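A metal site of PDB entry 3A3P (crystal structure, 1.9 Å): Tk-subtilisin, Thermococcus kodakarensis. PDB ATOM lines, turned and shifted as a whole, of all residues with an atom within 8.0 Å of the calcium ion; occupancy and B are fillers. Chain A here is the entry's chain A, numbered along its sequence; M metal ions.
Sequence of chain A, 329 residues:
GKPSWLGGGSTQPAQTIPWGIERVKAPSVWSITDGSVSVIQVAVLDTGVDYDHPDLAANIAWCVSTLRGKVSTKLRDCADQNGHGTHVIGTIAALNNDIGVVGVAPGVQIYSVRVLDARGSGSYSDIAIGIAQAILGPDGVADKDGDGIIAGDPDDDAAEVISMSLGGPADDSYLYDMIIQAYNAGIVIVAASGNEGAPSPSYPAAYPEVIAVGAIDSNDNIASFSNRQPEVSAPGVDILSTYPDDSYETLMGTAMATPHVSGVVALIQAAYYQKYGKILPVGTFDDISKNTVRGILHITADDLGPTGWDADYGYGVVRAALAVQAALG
NE2 of Gln 15 lies within hydrogen-bond range of OD1 of Asn 96 (3.0 Å). The backbone carbonyl oxygen (O) of Asp 98 lies within hydrogen-bond range of the backbone NH (N) of Gln 15, at 3.1 Å.
Within 4 Å of the calcium ion: Gln 15, Asp 55, Leu 95, Asn 97, Ile 99 and Val 101. The nearest printed residue that does not touch the calcium ion is Gly 100 (4.3 Å).
The calcium ion is bound by O of Val 101 (2.3 Å), O of Leu 95 (2.3 Å), OD1 of Asn 97 (2.4 Å), O of Ile 99 (2.4 Å), OD1 of Asp 55 (2.4 Å), OE1 of Gln 15 (2.5 Å) and OD2 of Asp 55 (2.6 Å). The calcium ion has seven donor atoms within binding distance.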
ATOM      1  N   GLN A  12      20.962  21.929  14.913  1.00  0.00           N
ATOM      2  CA  GLN A  12      20.625  20.603  15.576  1.00  0.00           C
ATOM      3  C   GLN A  12      21.672  20.152  16.591  1.00  0.00           C
ATOM      4  O   GLN A  12      22.861  20.194  16.299  1.00  0.00           O
ATOM      5  CB  GLN A  12      20.426  19.501  14.525  1.00  0.00           C
ATOM      6  CG  GLN A  12      19.201  19.697  13.647  1.00  0.00           C
ATOM      7  CD  GLN A  12      17.920  19.418  14.406  1.00  0.00           C
ATOM      8  OE1 GLN A  12      17.809  18.415  15.128  1.00  0.00           O
ATOM      9  NE2 GLN A  12      16.949  20.295  14.244  1.00  0.00           N
ATOM     10  N   PRO A  13      21.220  19.704  17.779  1.00  0.00           N
ATOM     11  CA  PRO A  13      22.140  19.199  18.813  1.00  0.00           C
ATOM     12  C   PRO A  13      22.715  17.824  18.433  1.00  0.00           C
ATOM     13  O   PRO A  13      22.045  17.064  17.735  1.00  0.00           O
ATOM     14  CB  PRO A  13      21.253  19.086  20.064  1.00  0.00           C
ATOM     15  CG  PRO A  13      19.882  18.861  19.517  1.00  0.00           C
ATOM     16  CD  PRO A  13      19.817  19.664  18.224  1.00  0.00           C
ATOM     17  N   ALA A  14      23.941  17.508  18.877  1.00  0.00           N
ATOM     18  CA  ALA A  14      24.504  16.169  18.738  1.00  0.00           C
ATOM     19  C   ALA A  14      23.577  15.107  19.363  1.00  0.00           C
ATOM     20  O   ALA A  14      22.889  15.395  20.320  1.00  0.00           O
ATOM     21  CB  ALA A  14      25.883  16.112  19.426  1.00  0.00           C
ATOM     22  N   GLN A  15      23.599  13.893  18.831  1.00  0.00           N
ATOM     23  CA  GLN A  15      22.651  12.864  19.255  1.00  0.00           C
ATOM     24  C   GLN A  15      22.927  12.348  20.654  1.00  0.00           C
ATOM     25  O   GLN A  15      24.092  12.112  20.983  1.00  0.00           O
ATOM     26  CB  GLN A  15      22.627  11.705  18.262  1.00  0.00           C
ATOM     27  CG  GLN A  15      21.716  10.541  18.703  1.00  0.00           C
ATOM     28  CD  GLN A  15      21.562   9.495  17.641  1.00  0.00           C
ATOM     29  OE1 GLN A  15      20.793   9.672  16.695  1.00  0.00           O
ATOM     30  NE2 GLN A  15      22.282   8.394  17.785  1.00  0.00           N
ATOM     31  N   THR A  16      21.877  12.197  21.458  1.00  0.00           N
ATOM     32  CA  THR A  16      21.921  11.377  22.679  1.00  0.00           C
ATOM     33  C   THR A  16      20.953  10.234  22.650  1.00  0.00           C
ATOM     34  O   THR A  16      19.945  10.299  21.939  1.00  0.00           O
ATOM     35  CB  THR A  16      21.415  12.077  23.987  1.00  0.00           C
ATOM     36  OG1 THR A  16      20.593  13.235  23.714  1.00  0.00           O
ATOM     37  CG2 THR A  16      22.493  12.334  24.918  1.00  0.00           C
ATOM     38  N   HIS A  53      10.569  17.114  10.455  1.00  0.00           N
ATOM     39  CA  HIS A  53      11.577  17.066  11.495  1.00  0.00           C
ATOM     40  C   HIS A  53      12.800  16.307  11.000  1.00  0.00           C
ATOM     41  O   HIS A  53      12.690  15.155  10.600  1.00  0.00           O
ATOM     42  CB  HIS A  53      11.050  16.416  12.802  1.00  0.00           C
ATOM     43  CG  HIS A  53      11.980  16.613  13.961  1.00  0.00           C
ATOM     44  ND1 HIS A  53      11.641  17.315  15.098  1.00  0.00           N
ATOM     45  CD2 HIS A  53      13.268  16.229  14.143  1.00  0.00           C
ATOM     46  CE1 HIS A  53      12.655  17.323  15.944  1.00  0.00           C
ATOM     47  NE2 HIS A  53      13.659  16.684  15.387  1.00  0.00           N
ATOM     48  N   PRO A  54      13.995  16.932  11.070  1.00  0.00           N
ATOM     49  CA  PRO A  54      15.210  16.287  10.595  1.00  0.00           C
ATOM     50  C   PRO A  54      15.469  14.907  11.239  1.00  0.00           C
ATOM     51  O   PRO A  54      16.102  14.038  10.617  1.00  0.00           O
ATOM     52  CB  PRO A  54      16.315  17.281  10.976  1.00  0.00           C
ATOM     53  CG  PRO A  54      15.652  18.628  11.046  1.00  0.00           C
ATOM     54  CD  PRO A  54      14.247  18.299  11.588  1.00  0.00           C
ATOM     55  N   ASP A  55      14.978  14.677  12.446  1.00  0.00           N
ATOM     56  CA  ASP A  55      15.263  13.405  13.121  1.00  0.00           C
ATOM     57  C   ASP A  55      14.141  12.383  12.989  1.00  0.00           C
ATOM     58  O   ASP A  55      14.174  11.309  13.620  1.00  0.00           O
ATOM     59  CB  ASP A  55      15.616  13.651  14.603  1.00  0.00           C
ATOM     60  CG  ASP A  55      16.702  12.724  15.100  1.00  0.00           C
ATOM     61  OD1 ASP A  55      17.525  12.257  14.284  1.00  0.00           O
ATOM     62  OD2 ASP A  55      16.759  12.454  16.308  1.00  0.00           O
ATOM     63  N   LEU A  56      13.151  12.728  12.165  1.00  0.00           N
ATOM     64  CA  LEU A  56      11.975  11.889  11.935  1.00  0.00           C
ATOM     65  C   LEU A  56      11.652  11.630  10.471  1.00  0.00           C
ATOM     66  O   LEU A  56      11.123  10.558  10.128  1.00  0.00           O
ATOM     67  CB  LEU A  56      10.735  12.534  12.561  1.00  0.00           C
ATOM     68  CG  LEU A  56      10.652  12.781  14.072  1.00  0.00           C
ATOM     69  CD1 LEU A  56       9.225  13.255  14.331  1.00  0.00           C
ATOM     70  CD2 LEU A  56      10.943  11.506  14.882  1.00  0.00           C
ATOM     71  N   ALA A  93      10.735   6.014  16.835  1.00  0.00           N
ATOM     72  CA  ALA A  93      11.405   5.949  15.525  1.00  0.00           C
ATOM     73  C   ALA A  93      12.319   7.114  15.176  1.00  0.00           C
ATOM     74  O   ALA A  93      12.634   7.288  13.992  1.00  0.00           O
ATOM     75  CB  ALA A  93      10.375   5.739  14.395  1.00  0.00           C
ATOM     76  N   ALA A  94      12.772   7.896  16.165  1.00  0.00           N
ATOM     77  CA  ALA A  94      13.797   8.930  15.843  1.00  0.00           C
ATOM     78  C   ALA A  94      15.027   8.238  15.269  1.00  0.00           C
ATOM     79  O   ALA A  94      15.408   7.186  15.732  1.00  0.00           O
ATOM     80  CB  ALA A  94      14.187   9.781  17.080  1.00  0.00           C
ATOM     81  N   LEU A  95      15.612   8.820  14.235  1.00  0.00           N
ATOM     82  CA  LEU A  95      16.639   8.161  13.446  1.00  0.00           C
ATOM     83  C   LEU A  95      17.943   8.053  14.241  1.00  0.00           C
ATOM     84  O   LEU A  95      18.233   8.915  15.081  1.00  0.00           O
ATOM     85  CB  LEU A  95      16.848   8.997  12.170  1.00  0.00           C
ATOM     86  CG  LEU A  95      15.671   8.931  11.203  1.00  0.00           C
ATOM     87  CD1 LEU A  95      15.532  10.229  10.354  1.00  0.00           C
ATOM     88  CD2 LEU A  95      15.807   7.714  10.333  1.00  0.00           C
ATOM     89  N   ASN A  96      18.711   7.011  13.974  1.00  0.00           N
ATOM     90  CA  ASN A  96      20.017   6.820  14.583  1.00  0.00           C
ATOM     91  C   ASN A  96      21.023   7.462  13.635  1.00  0.00           C
ATOM     92  O   ASN A  96      21.364   6.887  12.611  1.00  0.00           O
ATOM     93  CB  ASN A  96      20.304   5.340  14.722  1.00  0.00           C
ATOM     94  CG  ASN A  96      21.564   5.024  15.541  1.00  0.00           C
ATOM     95  OD1 ASN A  96      22.239   5.918  16.032  1.00  0.00           O
ATOM     96  ND2 ASN A  96      21.849   3.764  15.690  1.00  0.00           N
ATOM     97  N   ASN A  97      21.463   8.658  13.984  1.00  0.00           N
ATOM     98  CA  ASN A  97      22.283   9.502  13.088  1.00  0.00           C
ATOM     99  C   ASN A  97      23.173  10.379  13.965  1.00  0.00           C
ATOM    100  O   ASN A  97      23.516   9.979  15.079  1.00  0.00           O
ATOM    101  CB  ASN A  97      21.393  10.352  12.145  1.00  0.00           C
ATOM    102  CG  ASN A  97      20.309  11.159  12.891  1.00  0.00           C
ATOM    103  OD1 ASN A  97      20.400  11.397  14.086  1.00  0.00           O
ATOM    104  ND2 ASN A  97      19.291  11.609  12.159  1.00  0.00           N
ATOM    105  N   ASP A  98      23.500  11.582  13.519  1.00  0.00           N
ATOM    106  CA  ASP A  98      24.334  12.439  14.349  1.00  0.00           C
ATOM    107  C   ASP A  98      23.652  13.523  15.163  1.00  0.00           C
ATOM    108  O   ASP A  98      24.325  14.316  15.821  1.00  0.00           O
ATOM    109  CB  ASP A  98      25.530  12.951  13.543  1.00  0.00           C
ATOM    110  CG  ASP A  98      26.446  11.806  13.110  1.00  0.00           C
ATOM    111  OD1 ASP A  98      27.196  11.243  13.973  1.00  0.00           O
ATOM    112  OD2 ASP A  98      26.387  11.413  11.910  1.00  0.00           O
ATOM    113  N   ILE A  99      22.309  13.553  15.154  1.00  0.00           N
ATOM    114  CA  ILE A  99      21.566  14.617  15.814  1.00  0.00           C
ATOM    115  C   ILE A  99      20.454  14.110  16.756  1.00  0.00           C
ATOM    116  O   ILE A  99      19.984  12.979  16.651  1.00  0.00           O
ATOM    117  CB  ILE A  99      20.892  15.554  14.749  1.00  0.00           C
ATOM    118  CG1 ILE A  99      20.010  14.726  13.804  1.00  0.00           C
ATOM    119  CG2 ILE A  99      21.978  16.284  13.883  1.00  0.00           C
ATOM    120  CD1 ILE A  99      18.945  15.508  13.097  1.00  0.00           C
ATOM    121  N   GLY A 100      20.017  14.981  17.641  1.00  0.00           N
ATOM    122  CA  GLY A 100      18.765  14.796  18.358  1.00  0.00           C
ATOM    123  C   GLY A 100      18.749  13.595  19.272  1.00  0.00           C
ATOM    124  O   GLY A 100      19.560  13.469  20.199  1.00  0.00           O
ATOM    125  N   VAL A 101      17.765  12.732  19.067  1.00  0.00           N
ATOM    126  CA  VAL A 101      17.632  11.551  19.915  1.00  0.00           C
ATOM    127  C   VAL A 101      17.678  10.281  19.068  1.00  0.00           C
ATOM    128  O   VAL A 101      18.194  10.306  17.937  1.00  0.00           O
ATOM    129  CB  VAL A 101      16.348  11.639  20.771  1.00  0.00           C
ATOM    130  CG1 VAL A 101      16.468  12.793  21.791  1.00  0.00           C
ATOM    131  CG2 VAL A 101      15.107  11.813  19.877  1.00  0.00           C
ATOM    132  N   VAL A 102      17.168   9.150  19.574  1.00  0.00           N
ATOM    133  CA  VAL A 102      17.101   7.917  18.769  1.00  0.00           C
ATOM    134  C   VAL A 102      15.926   7.118  19.328  1.00  0.00           C
ATOM    135  O   VAL A 102      15.715   7.102  20.542  1.00  0.00           O
ATOM    136  CB  VAL A 102      18.452   7.101  18.729  1.00  0.00           C
ATOM    137  CG1 VAL A 102      18.991   6.736  20.137  1.00  0.00           C
ATOM    138  CG2 VAL A 102      18.358   5.821  17.864  1.00  0.00           C
ATOM    139  N   GLY A 103      15.114   6.519  18.438  1.00  0.00           N
ATOM    140  CA  GLY A 103      13.956   5.796  18.947  1.00  0.00           C
ATOM    141  C   GLY A 103      14.315   4.376  19.315  1.00  0.00           C
ATOM    142  O   GLY A 103      15.428   3.936  19.042  1.00  0.00           O
ATOM    143  N   PRO A 106      14.833   2.645  15.513  1.00  0.00           N
ATOM    144  CA  PRO A 106      15.173   3.847  14.758  1.00  0.00           C
ATOM    145  C   PRO A 106      15.095   3.731  13.211  1.00  0.00           C
ATOM    146  O   PRO A 106      15.281   4.752  12.513  1.00  0.00           O
ATOM    147  CB  PRO A 106      16.620   4.154  15.229  1.00  0.00           C
ATOM    148  CG  PRO A 106      17.161   2.913  15.730  1.00  0.00           C
ATOM    149  CD  PRO A 106      15.998   2.044  16.195  1.00  0.00           C
ATOM    150  N   THR A 242      11.632  14.092  20.261  1.00  0.00           N
ATOM    151  CA  THR A 242      11.397  15.138  19.280  1.00  0.00           C
ATOM    152  C   THR A 242      10.151  15.955  19.611  1.00  0.00           C
ATOM    153  O   THR A 242       9.190  15.477  20.238  1.00  0.00           O
ATOM    154  CB  THR A 242      11.245  14.513  17.877  1.00  0.00           C
ATOM    155  OG1 THR A 242      10.390  13.350  17.971  1.00  0.00           O
ATOM    156  CG2 THR A 242      12.621  14.063  17.331  1.00  0.00           C
ATOM    157  N   TYR A 248      13.236  19.524  20.392  1.00  0.00           N
ATOM    158  CA  TYR A 248      13.188  18.407  21.375  1.00  0.00           C
ATOM    159  C   TYR A 248      12.595  18.935  22.679  1.00  0.00           C
ATOM    160  O   TYR A 248      12.730  20.111  22.979  1.00  0.00           O
ATOM    161  CB  TYR A 248      14.596  17.827  21.598  1.00  0.00           C
ATOM    162  CG  TYR A 248      15.239  17.494  20.290  1.00  0.00           C
ATOM    163  CD1 TYR A 248      15.941  18.471  19.560  1.00  0.00           C
ATOM    164  CD2 TYR A 248      15.077  16.240  19.733  1.00  0.00           C
ATOM    165  CE1 TYR A 248      16.477  18.179  18.315  1.00  0.00           C
ATOM    166  CE2 TYR A 248      15.606  15.934  18.502  1.00  0.00           C
ATOM    167  CZ  TYR A 248      16.301  16.916  17.787  1.00  0.00           C
ATOM    168  OH  TYR A 248      16.819  16.575  16.545  1.00  0.00           O
HETATM  169 CA    CA M   1      18.911  11.019  15.872  1.00  0.00          CA
